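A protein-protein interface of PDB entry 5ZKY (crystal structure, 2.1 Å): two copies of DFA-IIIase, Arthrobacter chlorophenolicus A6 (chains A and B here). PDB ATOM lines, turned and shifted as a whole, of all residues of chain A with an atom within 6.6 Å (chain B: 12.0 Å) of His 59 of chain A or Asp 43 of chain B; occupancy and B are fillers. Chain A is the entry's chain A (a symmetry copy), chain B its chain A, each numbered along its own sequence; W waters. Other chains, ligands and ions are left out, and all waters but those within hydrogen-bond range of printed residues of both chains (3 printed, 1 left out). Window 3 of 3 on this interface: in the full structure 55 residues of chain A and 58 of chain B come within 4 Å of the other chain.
The indole nitrogen (NE1) of Trp 101 of chain A sits at hydrogen-bond distance from the side-chain carboxylate (OD1) of Asp 40 of chain B.
O of Asp 42 of chain B lies within hydrogen-bond range of NE2 of His 59 of chain A (2.9 Å).
The backbone carbonyl oxygen of Asp 43 of chain B lies within hydrogen-bond range of the guanidinium group of Arg 106 of chain A, 2.8 Å away.
The side-chain carboxylate (OD2) of Asp 57 of chain A sits at hydrogen-bond distance from the backbone NH (N) of Gly 45 of chain B (2.8 Å).
O of Ala 18 of chain A lies close to N of His 59 of chain A, at 3.2 Å.
The guanidinium group of Arg 106 of chain A is in salt-bridge range of the side-chain carboxylate of Asp 57 of chain A (2.8 Å).
N of Tyr 58 of chain A lies within hydrogen-bond range of O of Arg 106 of chain A (2.8 Å).
The backbone NH of Ile 108 of chain A is in hydrogen-bond range of the backbone carbonyl oxygen of Tyr 58 of chain A (2.7 Å).
The backbone NH (N) of Leu 60 of chain A lies within hydrogen-bond range of the backbone carbonyl oxygen (O) of Ile 108 of chain A.
The backbone carbonyl oxygen of Pro 102 of chain A lies close to the guanidinium group of Arg 106 of chain A, 3.2 Å away.
Among the printed residues, merely in contact across the chains: Asp 57 of chain A with Gly 44 of chain B (3.6 Å), Asp 57 of chain A with Pro 47 of chain B (3.5 Å), His 59 of chain A with Asp 43 of chain B (3.3 Å), Trp 101 of chain A with Ala 39 of chain B (3.4 Å), Trp 101 of chain A with Asp 43 of chain B (3.3 Å), Trp 101 of chain A with Gly 44 of chain B (3.5 Å), Trp 101 of chain A with Phe 70 of chain B (3.5 Å), Pro 102 of chain A with Phe 70 of chain B (3.96 Å), Arg 106 of chain A with Gly 44 of chain B (3.6 Å), Ile 108 of chain A with Asp 43 of chain B (3.999 Å) and Leu 148 of chain A with Asp 43 of chain B (3.7 Å).
His 59 of chain A touches just these residues of chain B: Asp 42 and Asp 43.
Printed residues of chain A within 4 Å of Asp 43 of chain B: His 59 (3.3 Å), Trp 101 (3.3 Å), Arg 106 (2.8 Å), Ile 108 (3.999 Å) and Leu 148 (3.7 Å).
No residue of chain B comes within 4 Å of Pro 17 of chain A.
Lys 19 of chain A touches none of the printed residues of chain B.
No residue of chain B comes within 4 Å of Asp 20 of chain A.
No residue of chain B comes within 4 Å of Ile 21 of chain A.
Asp 57 of chain A touches just these residues of chain B: Gly 44, Gly 45 and Pro 47.
No residue of chain B comes within 4 Å of Arg 61 of chain A.
Printed residues of chain B within 4 Å of Trp 101 of chain A: Ala 39 (3.4 Å), Asp 40 (2.8 Å), Asp 43 (3.3 Å), Gly 44 (3.5 Å) and Phe 70 (3.5 Å).
Pro 102 of chain A touches one residue of chain B.
Asp 110 of chain A touches none of the printed residues of chain B.
Of the printed residues of chain A, Pro 47 of chain B touches Asp 57 (3.5 Å).
Of the printed residues of chain A, Gly 44 of chain B touches Asp 57, Trp 101 and Arg 106.
Printed residues of chain B within 4 Å of Ile 108 of chain A: Asp 43 (3.999 Å).
The nearest printed residue of chain A that does not touch Asp 43 of chain B is Asp 110 of chain A (4.9 Å).
The nearest printed residue of chain A that does not touch Ala 39 of chain B is Asp 57 of chain A (7.3 Å).
Printed residues of chain B that touch a printed residue of chain A: Ala 39, Asp 40, Asp 42, Asp 43, Gly 44, Gly 45, Pro 47 and Phe 70.
Of the 23 printed residues of chain A, 7 touch a printed residue of chain B.
Printed residues of chain A that touch a printed residue of chain B: Asp 57, His 59, Trp 101, Pro 102, Arg 106, Ile 108 and Leu 148.
Hydrophobic or aromatic side chains of chain A that line the printed part of chain B: His 59, Trp 101, Ile 108 and Leu 148.
No position is printed for both chains.
Water W1 lies within hydrogen-bond range of O of Ala 39 of chain B and N of Trp 101 of chain A.
Water W2 lies within hydrogen-bond range of OD2 of Asp 57 of chain A (2.7 Å) and N of Gly 45 of chain B (3.5 Å).
Water W3 bridges the backbone carbonyl oxygen of Trp 101 of chain A (2.8 Å) and the backbone carbonyl oxygen of Lys 46 of chain B (3.1 Å).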
ATOM      1  N   ASN A  16     -24.058  17.046   1.820  1.00  0.00           N
ATOM      2  CA  ASN A  16     -24.663  16.432   0.663  1.00  0.00           C
ATOM      3  C   ASN A  16     -23.598  15.488   0.106  1.00  0.00           C
ATOM      4  O   ASN A  16     -22.552  15.960  -0.333  1.00  0.00           O
ATOM      5  CB  ASN A  16     -25.011  17.545  -0.328  1.00  0.00           C
ATOM      6  CG  ASN A  16     -25.616  17.027  -1.621  1.00  0.00           C
ATOM      7  OD1 ASN A  16     -25.474  15.853  -2.000  1.00  0.00           O
ATOM      8  ND2 ASN A  16     -26.295  17.916  -2.313  1.00  0.00           N
ATOM      9  N   PRO A  17     -23.844  14.158   0.148  1.00  0.00           N
ATOM     10  CA  PRO A  17     -22.818  13.212  -0.313  1.00  0.00           C
ATOM     11  C   PRO A  17     -22.525  13.244  -1.826  1.00  0.00           C
ATOM     12  O   PRO A  17     -21.427  12.836  -2.243  1.00  0.00           O
ATOM     13  CB  PRO A  17     -23.385  11.856   0.110  1.00  0.00           C
ATOM     14  CG  PRO A  17     -24.864  12.051   0.090  1.00  0.00           C
ATOM     15  CD  PRO A  17     -25.078  13.458   0.577  1.00  0.00           C
ATOM     16  N   ALA A  18     -23.480  13.714  -2.634  1.00  0.00           N
ATOM     17  CA  ALA A  18     -23.232  13.951  -4.047  1.00  0.00           C
ATOM     18  C   ALA A  18     -22.161  15.041  -4.255  1.00  0.00           C
ATOM     19  O   ALA A  18     -21.336  14.917  -5.166  1.00  0.00           O
ATOM     20  CB  ALA A  18     -24.537  14.325  -4.777  1.00  0.00           C
ATOM     21  N   LYS A  19     -22.161  16.080  -3.409  1.00  0.00           N
ATOM     22  CA  LYS A  19     -21.275  17.246  -3.567  1.00  0.00           C
ATOM     23  C   LYS A  19     -19.949  17.035  -2.828  1.00  0.00           C
ATOM     24  O   LYS A  19     -18.872  17.283  -3.376  1.00  0.00           O
ATOM     25  CB  LYS A  19     -21.967  18.533  -3.067  1.00  0.00           C
ATOM     26  N   ASP A  20     -20.024  16.587  -1.577  1.00  0.00           N
ATOM     27  CA  ASP A  20     -18.814  16.276  -0.805  1.00  0.00           C
ATOM     28  C   ASP A  20     -19.109  15.217   0.248  1.00  0.00           C
ATOM     29  O   ASP A  20     -19.429  15.529   1.390  1.00  0.00           O
ATOM     30  CB  ASP A  20     -18.207  17.547  -0.177  1.00  0.00           C
ATOM     31  CG  ASP A  20     -16.849  17.294   0.474  1.00  0.00           C
ATOM     32  OD1 ASP A  20     -16.320  16.153   0.389  1.00  0.00           O
ATOM     33  OD2 ASP A  20     -16.298  18.235   1.079  1.00  0.00           O
ATOM     34  N   ILE A  21     -19.004  13.955  -0.160  1.00  0.00           N
ATOM     35  CA  ILE A  21     -19.157  12.818   0.770  1.00  0.00           C
ATOM     36  C   ILE A  21     -18.095  12.795   1.874  1.00  0.00           C
ATOM     37  O   ILE A  21     -18.336  12.266   2.952  1.00  0.00           O
ATOM     38  CB  ILE A  21     -19.196  11.467   0.018  1.00  0.00           C
ATOM     39  CG1 ILE A  21     -19.677  10.346   0.940  1.00  0.00           C
ATOM     40  CG2 ILE A  21     -17.843  11.138  -0.616  1.00  0.00           C
ATOM     41  CD1 ILE A  21     -19.942   9.039   0.235  1.00  0.00           C
ATOM     42  N   GLY A  22     -16.925  13.366   1.603  1.00  0.00           N
ATOM     43  CA  GLY A  22     -15.885  13.539   2.612  1.00  0.00           C
ATOM     44  C   GLY A  22     -16.358  14.286   3.848  1.00  0.00           C
ATOM     45  O   GLY A  22     -16.128  13.845   4.975  1.00  0.00           O
ATOM     46  N   ASP A  57     -23.278   8.079  -7.195  1.00  0.00           N
ATOM     47  CA  ASP A  57     -22.108   8.837  -7.589  1.00  0.00           C
ATOM     48  C   ASP A  57     -21.843   9.927  -6.559  1.00  0.00           C
ATOM     49  O   ASP A  57     -22.554  10.918  -6.500  1.00  0.00           O
ATOM     50  CB  ASP A  57     -22.326   9.460  -8.967  1.00  0.00           C
ATOM     51  CG  ASP A  57     -22.470   8.425 -10.061  1.00  0.00           C
ATOM     52  OD1 ASP A  57     -21.579   7.551 -10.186  1.00  0.00           O
ATOM     53  OD2 ASP A  57     -23.466   8.504 -10.813  1.00  0.00           O
ATOM     54  N   TYR A  58     -20.794   9.748  -5.762  1.00  0.00           N
ATOM     55  CA  TYR A  58     -20.473  10.660  -4.677  1.00  0.00           C
ATOM     56  C   TYR A  58     -19.122  11.329  -4.911  1.00  0.00           C
ATOM     57  O   TYR A  58     -18.090  10.669  -4.988  1.00  0.00           O
ATOM     58  CB  TYR A  58     -20.457   9.903  -3.356  1.00  0.00           C
ATOM     59  CG  TYR A  58     -21.679   9.052  -3.102  1.00  0.00           C
ATOM     60  CD1 TYR A  58     -22.944   9.631  -2.913  1.00  0.00           C
ATOM     61  CD2 TYR A  58     -21.578   7.661  -3.033  1.00  0.00           C
ATOM     62  CE1 TYR A  58     -24.067   8.840  -2.659  1.00  0.00           C
ATOM     63  CE2 TYR A  58     -22.692   6.869  -2.785  1.00  0.00           C
ATOM     64  CZ  TYR A  58     -23.933   7.455  -2.588  1.00  0.00           C
ATOM     65  OH  TYR A  58     -25.049   6.666  -2.344  1.00  0.00           O
ATOM     66  N   HIS A  59     -19.134  12.646  -5.021  1.00  0.00           N
ATOM     67  CA  HIS A  59     -17.912  13.427  -5.101  1.00  0.00           C
ATOM     68  C   HIS A  59     -17.337  13.610  -3.701  1.00  0.00           C
ATOM     69  O   HIS A  59     -18.064  13.922  -2.760  1.00  0.00           O
ATOM     70  CB  HIS A  59     -18.176  14.786  -5.762  1.00  0.00           C
ATOM     71  CG  HIS A  59     -18.592  14.677  -7.192  1.00  0.00           C
ATOM     72  ND1 HIS A  59     -17.704  14.832  -8.237  1.00  0.00           N
ATOM     73  CD2 HIS A  59     -19.788  14.382  -7.751  1.00  0.00           C
ATOM     74  CE1 HIS A  59     -18.344  14.652  -9.379  1.00  0.00           C
ATOM     75  NE2 HIS A  59     -19.611  14.383  -9.112  1.00  0.00           N
ATOM     76  N   LEU A  60     -16.037  13.380  -3.574  1.00  0.00           N
ATOM     77  CA  LEU A  60     -15.312  13.642  -2.341  1.00  0.00           C
ATOM     78  C   LEU A  60     -14.380  14.824  -2.596  1.00  0.00           C
ATOM     79  O   LEU A  60     -13.472  14.747  -3.442  1.00  0.00           O
ATOM     80  CB  LEU A  60     -14.548  12.398  -1.908  1.00  0.00           C
ATOM     81  CG  LEU A  60     -13.702  12.507  -0.623  1.00  0.00           C
ATOM     82  CD1 LEU A  60     -13.735  11.201   0.168  1.00  0.00           C
ATOM     83  CD2 LEU A  60     -12.254  12.877  -0.944  1.00  0.00           C
ATOM     84  N   ARG A  61     -14.634  15.928  -1.886  1.00  0.00           N
ATOM     85  CA  ARG A  61     -13.792  17.139  -1.975  1.00  0.00           C
ATOM     86  C   ARG A  61     -12.985  17.397  -0.713  1.00  0.00           C
ATOM     87  O   ARG A  61     -12.133  18.265  -0.718  1.00  0.00           O
ATOM     88  CB  ARG A  61     -14.655  18.378  -2.330  1.00  0.00           C
ATOM     89  CG  ARG A  61     -15.450  18.177  -3.613  1.00  0.00           C
ATOM     90  CD  ARG A  61     -15.970  19.443  -4.284  1.00  0.00           C
ATOM     91  NE  ARG A  61     -15.973  19.175  -5.736  1.00  0.00           N
ATOM     92  CZ  ARG A  61     -16.954  18.595  -6.443  1.00  0.00           C
ATOM     93  NH1 ARG A  61     -16.772  18.378  -7.732  1.00  0.00           N
ATOM     94  NH2 ARG A  61     -18.128  18.249  -5.899  1.00  0.00           N
ATOM     95  N   THR A  62     -13.258  16.652   0.358  1.00  0.00           N
ATOM     96  CA  THR A  62     -12.517  16.757   1.609  1.00  0.00           C
ATOM     97  C   THR A  62     -12.053  15.355   2.000  1.00  0.00           C
ATOM     98  O   THR A  62     -12.841  14.407   2.002  1.00  0.00           O
ATOM     99  CB  THR A  62     -13.419  17.309   2.729  1.00  0.00           C
ATOM    100  OG1 THR A  62     -14.048  18.505   2.282  1.00  0.00           O
ATOM    101  CG2 THR A  62     -12.621  17.609   4.009  1.00  0.00           C
ATOM    102  N   TRP A 101     -18.749   5.853 -17.134  1.00  0.00           N
ATOM    103  CA  TRP A 101     -18.039   5.955 -15.875  1.00  0.00           C
ATOM    104  C   TRP A 101     -18.221   4.694 -15.043  1.00  0.00           C
ATOM    105  O   TRP A 101     -19.185   3.939 -15.253  1.00  0.00           O
ATOM    106  CB  TRP A 101     -18.595   7.128 -15.071  1.00  0.00           C
ATOM    107  CG  TRP A 101     -18.382   8.474 -15.699  1.00  0.00           C
ATOM    108  CD1 TRP A 101     -19.338   9.274 -16.236  1.00  0.00           C
ATOM    109  CD2 TRP A 101     -17.141   9.177 -15.843  1.00  0.00           C
ATOM    110  NE1 TRP A 101     -18.783  10.436 -16.700  1.00  0.00           N
ATOM    111  CE2 TRP A 101     -17.434  10.408 -16.478  1.00  0.00           C
ATOM    112  CE3 TRP A 101     -15.813   8.894 -15.495  1.00  0.00           C
ATOM    113  CZ2 TRP A 101     -16.443  11.364 -16.772  1.00  0.00           C
ATOM    114  CZ3 TRP A 101     -14.826   9.835 -15.786  1.00  0.00           C
ATOM    115  CH2 TRP A 101     -15.150  11.067 -16.413  1.00  0.00           C
ATOM    116  N   PRO A 102     -17.304   4.462 -14.079  1.00  0.00           N
ATOM    117  CA  PRO A 102     -17.542   3.476 -13.037  1.00  0.00           C
ATOM    118  C   PRO A 102     -18.808   3.810 -12.263  1.00  0.00           C
ATOM    119  O   PRO A 102     -19.358   4.923 -12.386  1.00  0.00           O
ATOM    120  CB  PRO A 102     -16.292   3.603 -12.149  1.00  0.00           C
ATOM    121  CG  PRO A 102     -15.228   4.079 -13.071  1.00  0.00           C
ATOM    122  CD  PRO A 102     -15.949   5.039 -13.964  1.00  0.00           C
ATOM    123  N   ARG A 106     -19.939   4.646  -5.369  1.00  0.00           N
ATOM    124  CA  ARG A 106     -18.780   5.273  -5.990  1.00  0.00           C
ATOM    125  C   ARG A 106     -18.329   6.571  -5.333  1.00  0.00           C
ATOM    126  O   ARG A 106     -19.076   7.556  -5.287  1.00  0.00           O
ATOM    127  CB  ARG A 106     -19.067   5.513  -7.467  1.00  0.00           C
ATOM    128  CG  ARG A 106     -17.981   6.210  -8.262  1.00  0.00           C
ATOM    129  CD  ARG A 106     -18.294   6.033  -9.737  1.00  0.00           C
ATOM    130  NE  ARG A 106     -17.461   6.840 -10.622  1.00  0.00           N
ATOM    131  CZ  ARG A 106     -17.870   7.870 -11.366  1.00  0.00           C
ATOM    132  NH1 ARG A 106     -19.138   8.276 -11.383  1.00  0.00           N
ATOM    133  NH2 ARG A 106     -16.982   8.497 -12.122  1.00  0.00           N
ATOM    134  N   VAL A 107     -17.083   6.558  -4.859  1.00  0.00           N
ATOM    135  CA  VAL A 107     -16.443   7.734  -4.300  1.00  0.00           C
ATOM    136  C   VAL A 107     -15.502   8.281  -5.360  1.00  0.00           C
ATOM    137  O   VAL A 107     -14.485   7.657  -5.700  1.00  0.00           O
ATOM    138  CB  VAL A 107     -15.687   7.392  -3.008  1.00  0.00           C
ATOM    139  CG1 VAL A 107     -14.919   8.608  -2.498  1.00  0.00           C
ATOM    140  CG2 VAL A 107     -16.665   6.873  -1.961  1.00  0.00           C
ATOM    141  N   ILE A 108     -15.876   9.435  -5.903  1.00  0.00           N
ATOM    142  CA  ILE A 108     -15.086  10.153  -6.891  1.00  0.00           C
ATOM    143  C   ILE A 108     -14.114  11.062  -6.144  1.00  0.00           C
ATOM    144  O   ILE A 108     -14.529  11.997  -5.460  1.00  0.00           O
ATOM    145  CB  ILE A 108     -15.990  11.000  -7.828  1.00  0.00           C
ATOM    146  CG1 ILE A 108     -16.966  10.093  -8.572  1.00  0.00           C
ATOM    147  CG2 ILE A 108     -15.152  11.802  -8.817  1.00  0.00           C
ATOM    148  CD1 ILE A 108     -18.169  10.821  -9.149  1.00  0.00           C
ATOM    149  N   VAL A 109     -12.822  10.808  -6.312  1.00  0.00           N
ATOM    150  CA  VAL A 109     -11.811  11.526  -5.565  1.00  0.00           C
ATOM    151  C   VAL A 109     -11.498  12.835  -6.300  1.00  0.00           C
ATOM    152  O   VAL A 109     -10.730  12.825  -7.265  1.00  0.00           O
ATOM    153  CB  VAL A 109     -10.542  10.669  -5.387  1.00  0.00           C
ATOM    154  CG1 VAL A 109      -9.553  11.370  -4.471  1.00  0.00           C
ATOM    155  CG2 VAL A 109     -10.915   9.292  -4.833  1.00  0.00           C
ATOM    156  N   ASP A 110     -12.118  13.935  -5.857  1.00  0.00           N
ATOM    157  CA  ASP A 110     -11.878  15.275  -6.414  1.00  0.00           C
ATOM    158  C   ASP A 110     -10.955  16.055  -5.466  1.00  0.00           C
ATOM    159  O   ASP A 110     -11.294  17.137  -5.029  1.00  0.00           O
ATOM    160  CB  ASP A 110     -13.192  16.057  -6.593  1.00  0.00           C
ATOM    161  CG  ASP A 110     -14.095  15.493  -7.679  1.00  0.00           C
ATOM    162  OD1 ASP A 110     -13.614  15.088  -8.749  1.00  0.00           O
ATOM    163  OD2 ASP A 110     -15.325  15.487  -7.473  1.00  0.00           O
ATOM    164  N   ASP A 146     -12.715   5.992  -7.212  1.00  0.00           N
ATOM    165  CA  ASP A 146     -12.464   6.360  -8.608  1.00  0.00           C
ATOM    166  C   ASP A 146     -11.721   7.687  -8.640  1.00  0.00           C
ATOM    167  O   ASP A 146     -12.244   8.702  -8.178  1.00  0.00           O
ATOM    168  CB  ASP A 146     -13.818   6.487  -9.314  1.00  0.00           C
ATOM    169  CG  ASP A 146     -13.719   6.761 -10.809  1.00  0.00           C
ATOM    170  OD1 ASP A 146     -12.610   6.883 -11.380  1.00  0.00           O
ATOM    171  OD2 ASP A 146     -14.808   6.858 -11.415  1.00  0.00           O
ATOM    172  N   LEU A 148     -10.994   9.143 -11.407  1.00  0.00           N
ATOM    173  CA  LEU A 148     -11.653   9.846 -12.504  1.00  0.00           C
ATOM    174  C   LEU A 148     -10.867  10.091 -13.801  1.00  0.00           C
ATOM    175  O   LEU A 148     -11.346   9.732 -14.871  1.00  0.00           O
ATOM    176  CB  LEU A 148     -12.238  11.182 -12.017  1.00  0.00           C
ATOM    177  CG  LEU A 148     -13.473  11.697 -12.761  1.00  0.00           C
ATOM    178  CD1 LEU A 148     -14.687  10.787 -12.542  1.00  0.00           C
ATOM    179  CD2 LEU A 148     -13.796  13.138 -12.333  1.00  0.00           C
ATOM    180  N   HIS A 149      -9.685  10.704 -13.687  1.00  0.00           N
ATOM    181  CA  HIS A 149      -8.808  11.023 -14.818  1.00  0.00           C
ATOM    182  C   HIS A 149      -7.352  10.816 -14.399  1.00  0.00           C
ATOM    183  O   HIS A 149      -6.985  11.049 -13.229  1.00  0.00           O
ATOM    184  CB  HIS A 149      -8.913  12.501 -15.279  1.00  0.00           C
ATOM    185  CG  HIS A 149     -10.254  12.888 -15.815  1.00  0.00           C
ATOM    186  ND1 HIS A 149     -10.657  12.588 -17.100  1.00  0.00           N
ATOM    187  CD2 HIS A 149     -11.275  13.578 -15.250  1.00  0.00           C
ATOM    188  CE1 HIS A 149     -11.881  13.053 -17.291  1.00  0.00           C
ATOM    189  NE2 HIS A 149     -12.280  13.653 -16.183  1.00  0.00           N
ATOM    190  N   ASN B   5     -31.130   4.199  -4.865  1.00  0.00           N
ATOM    191  CA  ASN B   5     -30.697   3.020  -5.661  1.00  0.00           C
ATOM    192  C   ASN B   5     -30.681   1.720  -4.846  1.00  0.00           C
ATOM    193  O   ASN B   5     -30.006   0.803  -5.252  1.00  0.00           O
ATOM    194  CB  ASN B   5     -29.371   3.278  -6.374  1.00  0.00           C
ATOM    195  CG  ASN B   5     -29.389   4.535  -7.207  1.00  0.00           C
ATOM    196  OD1 ASN B   5     -30.252   4.713  -8.040  1.00  0.00           O
ATOM    197  ND2 ASN B   5     -28.432   5.405  -6.980  1.00  0.00           N
ATOM    198  N   GLN B  36     -31.915   6.373 -14.430  1.00  0.00           N
ATOM    199  CA  GLN B  36     -30.502   6.488 -14.797  1.00  0.00           C
ATOM    200  C   GLN B  36     -30.353   6.489 -16.324  1.00  0.00           C
ATOM    201  O   GLN B  36     -29.711   5.605 -16.893  1.00  0.00           O
ATOM    202  CB  GLN B  36     -29.682   5.357 -14.130  1.00  0.00           C
ATOM    203  CG  GLN B  36     -29.771   5.375 -12.596  1.00  0.00           C
ATOM    204  CD  GLN B  36     -28.888   4.348 -11.893  1.00  0.00           C
ATOM    205  OE1 GLN B  36     -28.060   3.680 -12.519  1.00  0.00           O
ATOM    206  NE2 GLN B  36     -29.051   4.234 -10.564  1.00  0.00           N
ATOM    207  N   GLY B  37     -30.942   7.498 -16.972  1.00  0.00           N
ATOM    208  CA  GLY B  37     -30.937   7.619 -18.433  1.00  0.00           C
ATOM    209  C   GLY B  37     -29.691   8.289 -19.003  1.00  0.00           C
ATOM    210  O   GLY B  37     -29.259   7.952 -20.090  1.00  0.00           O
ATOM    211  N   ALA B  38     -29.103   9.236 -18.274  1.00  0.00           N
ATOM    212  CA  ALA B  38     -27.975  10.017 -18.785  1.00  0.00           C
ATOM    213  C   ALA B  38     -26.643   9.430 -18.288  1.00  0.00           C
ATOM    214  O   ALA B  38     -26.486   9.136 -17.102  1.00  0.00           O
ATOM    215  CB  ALA B  38     -28.120  11.482 -18.377  1.00  0.00           C
ATOM    216  N   ALA B  39     -25.694   9.292 -19.210  1.00  0.00           N
ATOM    217  CA  ALA B  39     -24.420   8.609 -18.988  1.00  0.00           C
ATOM    218  C   ALA B  39     -23.299   9.526 -18.454  1.00  0.00           C
ATOM    219  O   ALA B  39     -22.280   9.024 -17.950  1.00  0.00           O
ATOM    220  CB  ALA B  39     -23.979   7.917 -20.285  1.00  0.00           C
ATOM    221  N   ASP B  40     -23.485  10.849 -18.544  1.00  0.00           N
ATOM    222  CA  ASP B  40     -22.424  11.803 -18.219  1.00  0.00           C
ATOM    223  C   ASP B  40     -22.976  13.098 -17.646  1.00  0.00           C
ATOM    224  O   ASP B  40     -22.937  14.135 -18.294  1.00  0.00           O
ATOM    225  CB  ASP B  40     -21.568  12.087 -19.471  1.00  0.00           C
ATOM    226  CG  ASP B  40     -20.253  12.796 -19.148  1.00  0.00           C
ATOM    227  OD1 ASP B  40     -19.791  12.768 -17.991  1.00  0.00           O
ATOM    228  OD2 ASP B  40     -19.664  13.380 -20.065  1.00  0.00           O
ATOM    229  N   VAL B  41     -23.486  13.017 -16.424  1.00  0.00           N
ATOM    230  CA  VAL B  41     -23.962  14.170 -15.667  1.00  0.00           C
ATOM    231  C   VAL B  41     -23.132  14.205 -14.390  1.00  0.00           C
ATOM    232  O   VAL B  41     -23.138  13.235 -13.628  1.00  0.00           O
ATOM    233  CB  VAL B  41     -25.470  14.017 -15.344  1.00  0.00           C
ATOM    234  CG1 VAL B  41     -25.938  15.032 -14.292  1.00  0.00           C
ATOM    235  CG2 VAL B  41     -26.286  14.140 -16.630  1.00  0.00           C
ATOM    236  N   ASP B  42     -22.399  15.300 -14.164  1.00  0.00           N
ATOM    237  CA  ASP B  42     -21.544  15.450 -12.972  1.00  0.00           C
ATOM    238  C   ASP B  42     -20.609  14.244 -12.803  1.00  0.00           C
ATOM    239  O   ASP B  42     -20.535  13.665 -11.730  1.00  0.00           O
ATOM    240  CB  ASP B  42     -22.401  15.637 -11.698  1.00  0.00           C
ATOM    241  CG  ASP B  42     -23.235  16.911 -11.724  1.00  0.00           C
ATOM    242  OD1 ASP B  42     -22.877  17.866 -12.442  1.00  0.00           O
ATOM    243  OD2 ASP B  42     -24.261  16.962 -11.014  1.00  0.00           O
ATOM    244  N   ASP B  43     -19.941  13.861 -13.888  1.00  0.00           N
ATOM    245  CA  ASP B  43     -18.972  12.765 -13.906  1.00  0.00           C
ATOM    246  C   ASP B  43     -19.548  11.393 -13.548  1.00  0.00           C
ATOM    247  O   ASP B  43     -18.816  10.520 -13.084  1.00  0.00           O
ATOM    248  CB  ASP B  43     -17.803  13.084 -12.974  1.00  0.00           C
ATOM    249  CG  ASP B  43     -17.173  14.410 -13.275  1.00  0.00           C
ATOM    250  OD1 ASP B  43     -16.859  14.653 -14.456  1.00  0.00           O
ATOM    251  OD2 ASP B  43     -16.993  15.201 -12.331  1.00  0.00           O
ATOM    252  N   GLY B  44     -20.845  11.201 -13.785  1.00  0.00           N
ATOM    253  CA  GLY B  44     -21.527   9.958 -13.464  1.00  0.00           C
ATOM    254  C   GLY B  44     -22.869   9.882 -14.163  1.00  0.00           C
ATOM    255  O   GLY B  44     -23.044  10.459 -15.243  1.00  0.00           O
ATOM    256  N   GLY B  45     -23.795   9.142 -13.557  1.00  0.00           N
ATOM    257  CA  GLY B  45     -25.178   9.072 -14.013  1.00  0.00           C
ATOM    258  C   GLY B  45     -25.797   7.680 -14.052  1.00  0.00           C
ATOM    259  O   GLY B  45     -27.027   7.560 -13.941  1.00  0.00           O
ATOM    260  N   LYS B  46     -24.971   6.639 -14.202  1.00  0.00           N
ATOM    261  CA  LYS B  46     -25.467   5.250 -14.253  1.00  0.00           C
ATOM    262  C   LYS B  46     -24.739   4.378 -13.246  1.00  0.00           C
ATOM    263  O   LYS B  46     -24.087   3.416 -13.618  1.00  0.00           O
ATOM    264  CB  LYS B  46     -25.327   4.675 -15.661  1.00  0.00           C
ATOM    265  CG  LYS B  46     -26.174   5.399 -16.708  1.00  0.00           C
ATOM    266  CD  LYS B  46     -26.143   4.677 -18.047  1.00  0.00           C
ATOM    267  CE  LYS B  46     -27.163   5.251 -19.024  1.00  0.00           C
ATOM    268  NZ  LYS B  46     -27.325   4.327 -20.177  1.00  0.00           N
ATOM    269  N   PRO B  47     -24.857   4.711 -11.954  1.00  0.00           N
ATOM    270  CA  PRO B  47     -24.115   3.970 -10.931  1.00  0.00           C
ATOM    271  C   PRO B  47     -24.675   2.568 -10.613  1.00  0.00           C
ATOM    272  O   PRO B  47     -24.020   1.788  -9.902  1.00  0.00           O
ATOM    273  CB  PRO B  47     -24.213   4.886  -9.710  1.00  0.00           C
ATOM    274  CG  PRO B  47     -25.503   5.602  -9.892  1.00  0.00           C
ATOM    275  CD  PRO B  47     -25.605   5.836 -11.375  1.00  0.00           C
ATOM    276  N   GLY B  48     -25.867   2.256 -11.125  1.00  0.00           N
ATOM    277  CA  GLY B  48     -26.494   0.970 -10.890  1.00  0.00           C
ATOM    278  C   GLY B  48     -27.281   0.999  -9.600  1.00  0.00           C
ATOM    279  O   GLY B  48     -27.784   2.042  -9.175  1.00  0.00           O
ATOM    280  N   PHE B  70     -23.201  -2.744 -13.025  1.00  0.00           N
ATOM    281  CA  PHE B  70     -23.185  -2.381 -11.618  1.00  0.00           C
ATOM    282  C   PHE B  70     -24.495  -2.686 -10.886  1.00  0.00           C
ATOM    283  O   PHE B  70     -24.859  -1.962  -9.957  1.00  0.00           O
ATOM    284  CB  PHE B  70     -22.807  -0.897 -11.414  1.00  0.00           C
ATOM    285  CG  PHE B  70     -21.858  -0.348 -12.445  1.00  0.00           C
ATOM    286  CD1 PHE B  70     -20.634  -0.952 -12.677  1.00  0.00           C
ATOM    287  CD2 PHE B  70     -22.191   0.797 -13.165  1.00  0.00           C
ATOM    288  CE1 PHE B  70     -19.768  -0.439 -13.628  1.00  0.00           C
ATOM    289  CE2 PHE B  70     -21.327   1.327 -14.109  1.00  0.00           C
ATOM    290  CZ  PHE B  70     -20.113   0.701 -14.348  1.00  0.00           C
HETATM  291  O   HOH W   1     -21.783   6.482 -17.310  1.00  0.00           O
HETATM  292  O   HOH W   2     -25.187  10.611 -10.724  1.00  0.00           O
HETATM  293  O   HOH W   3     -21.846   4.831 -15.249  1.00  0.00           O
